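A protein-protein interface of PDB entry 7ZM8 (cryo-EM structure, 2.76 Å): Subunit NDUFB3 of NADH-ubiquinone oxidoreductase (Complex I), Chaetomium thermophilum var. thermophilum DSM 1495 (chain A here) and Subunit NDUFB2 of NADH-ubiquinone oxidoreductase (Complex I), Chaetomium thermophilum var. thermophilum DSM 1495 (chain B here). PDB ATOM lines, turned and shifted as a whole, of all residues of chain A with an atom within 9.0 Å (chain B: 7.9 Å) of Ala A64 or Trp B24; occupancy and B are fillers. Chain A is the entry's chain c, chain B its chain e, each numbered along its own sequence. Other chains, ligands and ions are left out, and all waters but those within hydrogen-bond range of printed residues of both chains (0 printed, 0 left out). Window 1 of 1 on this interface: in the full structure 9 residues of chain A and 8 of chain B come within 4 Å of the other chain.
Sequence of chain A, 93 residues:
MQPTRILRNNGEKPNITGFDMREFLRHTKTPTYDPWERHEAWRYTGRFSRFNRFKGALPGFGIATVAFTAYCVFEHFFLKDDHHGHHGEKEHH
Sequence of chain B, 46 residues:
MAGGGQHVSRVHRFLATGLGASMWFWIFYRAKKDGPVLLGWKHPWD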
ATOM      1  N   ALA A  57      25.470  -1.058  -2.169  1.00  0.00           N
ATOM      2  CA  ALA A  57      26.104  -0.976  -3.479  1.00  0.00           C
ATOM      3  C   ALA A  57      25.972   0.415  -4.085  1.00  0.00           C
ATOM      4  O   ALA A  57      26.776   0.795  -4.942  1.00  0.00           O
ATOM      5  CB  ALA A  57      25.513  -2.026  -4.415  1.00  0.00           C
ATOM      6  N   LEU A  58      24.975   1.186  -3.658  1.00  0.00           N
ATOM      7  CA  LEU A  58      24.774   2.561  -4.114  1.00  0.00           C
ATOM      8  C   LEU A  58      24.778   3.438  -2.871  1.00  0.00           C
ATOM      9  O   LEU A  58      23.713   3.744  -2.314  1.00  0.00           O
ATOM     10  CB  LEU A  58      23.467   2.714  -4.891  1.00  0.00           C
ATOM     11  CG  LEU A  58      23.424   2.345  -6.374  1.00  0.00           C
ATOM     12  CD1 LEU A  58      24.335   3.248  -7.184  1.00  0.00           C
ATOM     13  CD2 LEU A  58      23.749   0.884  -6.619  1.00  0.00           C
ATOM     14  N   PRO A  59      25.952   3.852  -2.395  1.00  0.00           N
ATOM     15  CA  PRO A  59      26.048   4.489  -1.073  1.00  0.00           C
ATOM     16  C   PRO A  59      25.126   5.676  -0.837  1.00  0.00           C
ATOM     17  O   PRO A  59      24.300   5.640   0.079  1.00  0.00           O
ATOM     18  CB  PRO A  59      27.521   4.925  -1.009  1.00  0.00           C
ATOM     19  CG  PRO A  59      28.108   4.622  -2.373  1.00  0.00           C
ATOM     20  CD  PRO A  59      27.278   3.538  -2.940  1.00  0.00           C
ATOM     21  N   GLY A  60      25.239   6.720  -1.640  1.00  0.00           N
ATOM     22  CA  GLY A  60      24.499   7.926  -1.345  1.00  0.00           C
ATOM     23  C   GLY A  60      23.111   8.010  -1.933  1.00  0.00           C
ATOM     24  O   GLY A  60      22.476   9.062  -1.824  1.00  0.00           O
ATOM     25  N   PHE A  61      22.616   6.939  -2.551  1.00  0.00           N
ATOM     26  CA  PHE A  61      21.348   7.019  -3.265  1.00  0.00           C
ATOM     27  C   PHE A  61      20.184   7.292  -2.323  1.00  0.00           C
ATOM     28  O   PHE A  61      19.298   8.093  -2.637  1.00  0.00           O
ATOM     29  CB  PHE A  61      21.109   5.734  -4.049  1.00  0.00           C
ATOM     30  CG  PHE A  61      20.301   5.929  -5.293  1.00  0.00           C
ATOM     31  CD1 PHE A  61      20.916   6.247  -6.487  1.00  0.00           C
ATOM     32  CD2 PHE A  61      18.923   5.799  -5.267  1.00  0.00           C
ATOM     33  CE1 PHE A  61      20.173   6.431  -7.636  1.00  0.00           C
ATOM     34  CE2 PHE A  61      18.175   5.980  -6.410  1.00  0.00           C
ATOM     35  CZ  PHE A  61      18.801   6.297  -7.598  1.00  0.00           C
ATOM     36  N   GLY A  62      20.158   6.628  -1.168  1.00  0.00           N
ATOM     37  CA  GLY A  62      19.038   6.802  -0.258  1.00  0.00           C
ATOM     38  C   GLY A  62      18.950   8.203   0.317  1.00  0.00           C
ATOM     39  O   GLY A  62      17.867   8.787   0.387  1.00  0.00           O
ATOM     40  N   ILE A  63      20.084   8.755   0.746  1.00  0.00           N
ATOM     41  CA  ILE A  63      20.087  10.104   1.298  1.00  0.00           C
ATOM     42  C   ILE A  63      19.779  11.120   0.211  1.00  0.00           C
ATOM     43  O   ILE A  63      19.086  12.116   0.447  1.00  0.00           O
ATOM     44  CB  ILE A  63      21.432  10.401   1.990  1.00  0.00           C
ATOM     45  CG1 ILE A  63      21.660   9.460   3.179  1.00  0.00           C
ATOM     46  CG2 ILE A  63      21.498  11.848   2.443  1.00  0.00           C
ATOM     47  CD1 ILE A  63      22.358   8.157   2.832  1.00  0.00           C
ATOM     48  N   ALA A  64      20.280  10.881  -1.000  1.00  0.00           N
ATOM     49  CA  ALA A  64      20.097  11.841  -2.081  1.00  0.00           C
ATOM     50  C   ALA A  64      18.667  11.828  -2.607  1.00  0.00           C
ATOM     51  O   ALA A  64      18.131  12.877  -2.981  1.00  0.00           O
ATOM     52  CB  ALA A  64      21.087  11.550  -3.204  1.00  0.00           C
ATOM     53  N   THR A  65      18.038  10.654  -2.652  1.00  0.00           N
ATOM     54  CA  THR A  65      16.700  10.552  -3.227  1.00  0.00           C
ATOM     55  C   THR A  65      15.695  11.374  -2.433  1.00  0.00           C
ATOM     56  O   THR A  65      14.916  12.145  -3.005  1.00  0.00           O
ATOM     57  CB  THR A  65      16.266   9.088  -3.292  1.00  0.00           C
ATOM     58  OG1 THR A  65      17.186   8.352  -4.107  1.00  0.00           O
ATOM     59  CG2 THR A  65      14.871   8.974  -3.883  1.00  0.00           C
ATOM     60  N   VAL A  66      15.697  11.226  -1.108  1.00  0.00           N
ATOM     61  CA  VAL A  66      14.774  12.000  -0.285  1.00  0.00           C
ATOM     62  C   VAL A  66      15.150  13.476  -0.304  1.00  0.00           C
ATOM     63  O   VAL A  66      14.274  14.352  -0.295  1.00  0.00           O
ATOM     64  CB  VAL A  66      14.720  11.430   1.147  1.00  0.00           C
ATOM     65  CG1 VAL A  66      16.063  11.569   1.846  1.00  0.00           C
ATOM     66  CG2 VAL A  66      13.624  12.115   1.947  1.00  0.00           C
ATOM     67  N   ALA A  67      16.450  13.781  -0.333  1.00  0.00           N
ATOM     68  CA  ALA A  67      16.880  15.173  -0.390  1.00  0.00           C
ATOM     69  C   ALA A  67      16.460  15.831  -1.697  1.00  0.00           C
ATOM     70  O   ALA A  67      16.030  16.991  -1.705  1.00  0.00           O
ATOM     71  CB  ALA A  67      18.394  15.264  -0.207  1.00  0.00           C
ATOM     72  N   PHE A  68      16.578  15.109  -2.814  1.00  0.00           N
ATOM     73  CA  PHE A  68      16.205  15.684  -4.100  1.00  0.00           C
ATOM     74  C   PHE A  68      14.701  15.907  -4.203  1.00  0.00           C
ATOM     75  O   PHE A  68      14.263  16.838  -4.886  1.00  0.00           O
ATOM     76  CB  PHE A  68      16.686  14.789  -5.241  1.00  0.00           C
ATOM     77  CG  PHE A  68      16.534  15.410  -6.597  1.00  0.00           C
ATOM     78  CD1 PHE A  68      17.406  16.396  -7.020  1.00  0.00           C
ATOM     79  CD2 PHE A  68      15.522  15.009  -7.449  1.00  0.00           C
ATOM     80  CE1 PHE A  68      17.269  16.971  -8.265  1.00  0.00           C
ATOM     81  CE2 PHE A  68      15.383  15.580  -8.695  1.00  0.00           C
ATOM     82  CZ  PHE A  68      16.257  16.564  -9.102  1.00  0.00           C
ATOM     83  N   THR A  69      13.899  15.066  -3.546  1.00  0.00           N
ATOM     84  CA  THR A  69      12.457  15.286  -3.539  1.00  0.00           C
ATOM     85  C   THR A  69      12.100  16.557  -2.783  1.00  0.00           C
ATOM     86  O   THR A  69      11.143  17.253  -3.141  1.00  0.00           O
ATOM     87  CB  THR A  69      11.734  14.086  -2.931  1.00  0.00           C
ATOM     88  OG1 THR A  69      12.265  13.816  -1.629  1.00  0.00           O
ATOM     89  CG2 THR A  69      11.898  12.859  -3.815  1.00  0.00           C
ATOM     90  N   ALA A  70      12.852  16.872  -1.726  1.00  0.00           N
ATOM     91  CA  ALA A  70      12.622  18.119  -1.006  1.00  0.00           C
ATOM     92  C   ALA A  70      12.851  19.323  -1.911  1.00  0.00           C
ATOM     93  O   ALA A  70      12.073  20.283  -1.890  1.00  0.00           O
ATOM     94  CB  ALA A  70      13.525  18.192   0.224  1.00  0.00           C
ATOM     95  N   TYR A  71      13.916  19.291  -2.712  1.00  0.00           N
ATOM     96  CA  TYR A  71      14.136  20.360  -3.678  1.00  0.00           C
ATOM     97  C   TYR A  71      13.113  20.303  -4.804  1.00  0.00           C
ATOM     98  O   TYR A  71      12.704  21.344  -5.331  1.00  0.00           O
ATOM     99  CB  TYR A  71      15.554  20.280  -4.241  1.00  0.00           C
ATOM    100  CG  TYR A  71      15.796  21.223  -5.396  1.00  0.00           C
ATOM    101  CD1 TYR A  71      16.066  22.566  -5.174  1.00  0.00           C
ATOM    102  CD2 TYR A  71      15.745  20.773  -6.709  1.00  0.00           C
ATOM    103  CE1 TYR A  71      16.285  23.431  -6.226  1.00  0.00           C
ATOM    104  CE2 TYR A  71      15.961  21.631  -7.765  1.00  0.00           C
ATOM    105  CZ  TYR A  71      16.230  22.959  -7.518  1.00  0.00           C
ATOM    106  OH  TYR A  71      16.446  23.819  -8.571  1.00  0.00           O
ATOM    107  N   CYS A  72      12.694  19.097  -5.192  1.00  0.00           N
ATOM    108  CA  CYS A  72      11.748  18.961  -6.294  1.00  0.00           C
ATOM    109  C   CYS A  72      10.411  19.604  -5.957  1.00  0.00           C
ATOM    110  O   CYS A  72       9.725  20.127  -6.843  1.00  0.00           O
ATOM    111  CB  CYS A  72      11.560  17.487  -6.650  1.00  0.00           C
ATOM    112  SG  CYS A  72      10.570  17.200  -8.135  1.00  0.00           S
ATOM    113  N   THR B  17      29.420   7.882   2.202  1.00  0.00           N
ATOM    114  CA  THR B  17      28.051   8.204   1.823  1.00  0.00           C
ATOM    115  C   THR B  17      27.908   9.661   1.407  1.00  0.00           C
ATOM    116  O   THR B  17      27.027   9.989   0.607  1.00  0.00           O
ATOM    117  CB  THR B  17      27.089   7.875   2.965  1.00  0.00           C
ATOM    118  OG1 THR B  17      25.740   8.041   2.512  1.00  0.00           O
ATOM    119  CG2 THR B  17      27.333   8.773   4.165  1.00  0.00           C
ATOM    120  N   LEU B  19      30.229  11.386  -0.309  1.00  0.00           N
ATOM    121  CA  LEU B  19      30.673  11.408  -1.695  1.00  0.00           C
ATOM    122  C   LEU B  19      29.636  10.776  -2.606  1.00  0.00           C
ATOM    123  O   LEU B  19      29.443  11.224  -3.742  1.00  0.00           O
ATOM    124  CB  LEU B  19      32.013  10.696  -1.827  1.00  0.00           C
ATOM    125  CG  LEU B  19      33.169  11.528  -1.284  1.00  0.00           C
ATOM    126  CD1 LEU B  19      34.419  10.691  -1.112  1.00  0.00           C
ATOM    127  CD2 LEU B  19      33.417  12.716  -2.186  1.00  0.00           C
ATOM    128  N   GLY B  20      28.977   9.720  -2.133  1.00  0.00           N
ATOM    129  CA  GLY B  20      27.884   9.144  -2.894  1.00  0.00           C
ATOM    130  C   GLY B  20      26.698  10.080  -3.006  1.00  0.00           C
ATOM    131  O   GLY B  20      26.114  10.227  -4.081  1.00  0.00           O
ATOM    132  N   ALA B  21      26.324  10.722  -1.900  1.00  0.00           N
ATOM    133  CA  ALA B  21      25.254  11.708  -1.944  1.00  0.00           C
ATOM    134  C   ALA B  21      25.662  12.969  -2.694  1.00  0.00           C
ATOM    135  O   ALA B  21      24.793  13.770  -3.048  1.00  0.00           O
ATOM    136  CB  ALA B  21      24.804  12.065  -0.528  1.00  0.00           C
ATOM    137  N   SER B  22      26.959  13.169  -2.934  1.00  0.00           N
ATOM    138  CA  SER B  22      27.374  14.222  -3.852  1.00  0.00           C
ATOM    139  C   SER B  22      26.822  13.959  -5.245  1.00  0.00           C
ATOM    140  O   SER B  22      26.166  14.819  -5.838  1.00  0.00           O
ATOM    141  CB  SER B  22      28.897  14.329  -3.875  1.00  0.00           C
ATOM    142  OG  SER B  22      29.384  14.913  -2.680  1.00  0.00           O
ATOM    143  N   MET B  23      27.068  12.739  -5.741  1.00  0.00           N
ATOM    144  CA  MET B  23      26.436  12.310  -7.013  1.00  0.00           C
ATOM    145  C   MET B  23      24.989  12.000  -6.640  1.00  0.00           C
ATOM    146  O   MET B  23      24.666  12.082  -5.445  1.00  0.00           O
ATOM    147  CB  MET B  23      27.027  10.987  -7.498  1.00  0.00           C
ATOM    148  CG  MET B  23      28.355  11.076  -8.189  1.00  0.00           C
ATOM    149  SD  MET B  23      28.705   9.449  -8.901  1.00  0.00           S
ATOM    150  CE  MET B  23      27.939   8.388  -7.678  1.00  0.00           C
ATOM    151  N   TRP B  24      24.127  11.726  -7.612  1.00  0.00           N
ATOM    152  CA  TRP B  24      22.732  11.320  -7.293  1.00  0.00           C
ATOM    153  C   TRP B  24      22.007  12.540  -6.734  1.00  0.00           C
ATOM    154  O   TRP B  24      20.907  12.384  -6.206  1.00  0.00           O
ATOM    155  CB  TRP B  24      22.652  10.094  -6.368  1.00  0.00           C
ATOM    156  CG  TRP B  24      23.428   8.897  -6.824  1.00  0.00           C
ATOM    157  CD1 TRP B  24      24.304   8.164  -6.078  1.00  0.00           C
ATOM    158  CD2 TRP B  24      23.403   8.286  -8.127  1.00  0.00           C
ATOM    159  NE1 TRP B  24      24.822   7.140  -6.821  1.00  0.00           N
ATOM    160  CE2 TRP B  24      24.289   7.189  -8.083  1.00  0.00           C
ATOM    161  CE3 TRP B  24      22.720   8.549  -9.319  1.00  0.00           C
ATOM    162  CZ2 TRP B  24      24.512   6.368  -9.186  1.00  0.00           C
ATOM    163  CZ3 TRP B  24      22.941   7.737 -10.409  1.00  0.00           C
ATOM    164  CH2 TRP B  24      23.824   6.660 -10.340  1.00  0.00           C
ATOM    165  N   PHE B  25      22.663  13.690  -6.719  1.00  0.00           N
ATOM    166  CA  PHE B  25      21.967  14.948  -6.366  1.00  0.00           C
ATOM    167  C   PHE B  25      22.334  15.821  -7.549  1.00  0.00           C
ATOM    168  O   PHE B  25      21.441  16.430  -8.147  1.00  0.00           O
ATOM    169  CB  PHE B  25      22.426  15.523  -5.028  1.00  0.00           C
ATOM    170  CG  PHE B  25      21.552  16.653  -4.551  1.00  0.00           C
ATOM    171  CD1 PHE B  25      20.359  16.397  -3.894  1.00  0.00           C
ATOM    172  CD2 PHE B  25      21.900  17.974  -4.791  1.00  0.00           C
ATOM    173  CE1 PHE B  25      19.547  17.434  -3.467  1.00  0.00           C
ATOM    174  CE2 PHE B  25      21.085  19.009  -4.364  1.00  0.00           C
ATOM    175  CZ  PHE B  25      19.911  18.739  -3.703  1.00  0.00           C
ATOM    176  N   TRP B  26      23.626  15.831  -7.879  1.00  0.00           N
ATOM    177  CA  TRP B  26      24.082  16.533  -9.100  1.00  0.00           C
ATOM    178  C   TRP B  26      23.457  15.802 -10.281  1.00  0.00           C
ATOM    179  O   TRP B  26      22.981  16.473 -11.194  1.00  0.00           O
ATOM    180  CB  TRP B  26      25.608  16.465  -9.159  1.00  0.00           C
ATOM    181  CG  TRP B  26      26.239  17.182 -10.312  1.00  0.00           C
ATOM    182  CD1 TRP B  26      26.964  16.628 -11.327  1.00  0.00           C
ATOM    183  CD2 TRP B  26      26.225  18.600 -10.556  1.00  0.00           C
ATOM    184  NE1 TRP B  26      27.398  17.601 -12.185  1.00  0.00           N
ATOM    185  CE2 TRP B  26      26.962  18.820 -11.738  1.00  0.00           C
ATOM    186  CE3 TRP B  26      25.667  19.700  -9.896  1.00  0.00           C
ATOM    187  CZ2 TRP B  26      27.145  20.093 -12.271  1.00  0.00           C
ATOM    188  CZ3 TRP B  26      25.848  20.957 -10.425  1.00  0.00           C
ATOM    189  CH2 TRP B  26      26.578  21.148 -11.598  1.00  0.00           C
ATOM    190  N   ILE B  27      23.432  14.470 -10.224  1.00  0.00           N
ATOM    191  CA  ILE B  27      22.910  13.660 -11.363  1.00  0.00           C
ATOM    192  C   ILE B  27      21.463  14.070 -11.661  1.00  0.00           C
ATOM    193  O   ILE B  27      21.200  14.431 -12.819  1.00  0.00           O
ATOM    194  CB  ILE B  27      23.061  12.150 -11.092  1.00  0.00           C
ATOM    195  CG1 ILE B  27      24.531  11.757 -10.929  1.00  0.00           C
ATOM    196  CG2 ILE B  27      22.386  11.333 -12.182  1.00  0.00           C
ATOM    197  CD1 ILE B  27      25.407  12.170 -12.086  1.00  0.00           C
ATOM    198  N   PHE B  28      20.563  14.013 -10.673  1.00  0.00           N
ATOM    199  CA  PHE B  28      19.184  14.363 -10.982  1.00  0.00           C
ATOM    200  C   PHE B  28      18.965  15.863 -11.096  1.00  0.00           C
ATOM    201  O   PHE B  28      18.032  16.287 -11.784  1.00  0.00           O
ATOM    202  CB  PHE B  28      18.212  13.752  -9.971  1.00  0.00           C
ATOM    203  CG  PHE B  28      18.606  12.394  -9.483  1.00  0.00           C
ATOM    204  CD1 PHE B  28      18.788  11.356 -10.376  1.00  0.00           C
ATOM    205  CD2 PHE B  28      18.701  12.125  -8.140  1.00  0.00           C
ATOM    206  CE1 PHE B  28      19.126  10.094  -9.936  1.00  0.00           C
ATOM    207  CE2 PHE B  28      19.029  10.859  -7.694  1.00  0.00           C
ATOM    208  CZ  PHE B  28      19.248   9.849  -8.588  1.00  0.00           C
ATOM    209  N   TYR B  29      19.780  16.684 -10.438  1.00  0.00           N
ATOM    210  CA  TYR B  29      19.692  18.116 -10.700  1.00  0.00           C
ATOM    211  C   TYR B  29      20.071  18.426 -12.137  1.00  0.00           C
ATOM    212  O   TYR B  29      19.433  19.255 -12.793  1.00  0.00           O
ATOM    213  CB  TYR B  29      20.581  18.900  -9.744  1.00  0.00           C
ATOM    214  CG  TYR B  29      20.392  20.390  -9.868  1.00  0.00           C
ATOM    215  CD1 TYR B  29      19.142  20.964  -9.676  1.00  0.00           C
ATOM    216  CD2 TYR B  29      21.450  21.220 -10.194  1.00  0.00           C
ATOM    217  CE1 TYR B  29      18.958  22.321  -9.792  1.00  0.00           C
ATOM    218  CE2 TYR B  29      21.276  22.582 -10.311  1.00  0.00           C
ATOM    219  CZ  TYR B  29      20.026  23.127 -10.110  1.00  0.00           C
ATOM    220  OH  TYR B  29      19.841  24.485 -10.227  1.00  0.00           O
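OG1 of Thr A65 is in hydrogen-bond range of O of Phe A61, 2.6 Å away.
Among the printed residues, pairs that only touch across the chains: Ala A64 with Trp B24 (3.1 Å), Tyr A71 with Tyr B29 (3.2 Å), Phe A68 with Phe B28 (3.2 Å), Phe A68 with Tyr B29 (3.3 Å), Gly A60 with Ala B21 (3.4 Å), Ile A63 with Thr B17 (3.4 Å), Gly A60 with Gly B20 (3.5 Å), Phe A61 with Trp B24 (3.6 Å), Phe A61 with Phe B28 (3.7 Å), Pro A59 with Thr B17 (3.7 Å), Leu A58 with Trp B24 (3.7 Å), Gly A60 with Thr B17 (3.8 Å), Phe A68 with Phe B25 (3.8 Å) and Ala A67 with Phe B25 (3.9 Å).
Trp B24 touches just these residues of chain A: Leu A58, Phe A61 and Ala A64.
Printed residues of chain B within 4 Å of Ile A63: Thr B17.
Printed residues of chain A within 4 Å of Phe B25: Ala A67 and Phe A68.
Of the printed residues of chain B, Phe A61 touches Trp B24 and Phe B28.
Printed residues of chain A within 4 Å of Phe B28: Phe A61 (3.7 Å) and Phe A68 (3.2 Å).
The nearest printed residue of chain B that does not touch Ala A64 is Met B23 (4.3 Å).
Hydrophobic or aromatic side chains of chain B within 4 Å of the printed part of chain A: Trp B24, Phe B25, Phe B28 and Tyr B29.
Hydrophobic or aromatic side chains of chain A that line the printed part of chain B: Leu A58, Phe A61, Ile A63, Ala A64, Phe A68 and Tyr A71.
Among the printed residues, no Asp or Glu carboxylate lies within 4 Å of a Lys or Arg side-chain nitrogen of the other chain.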
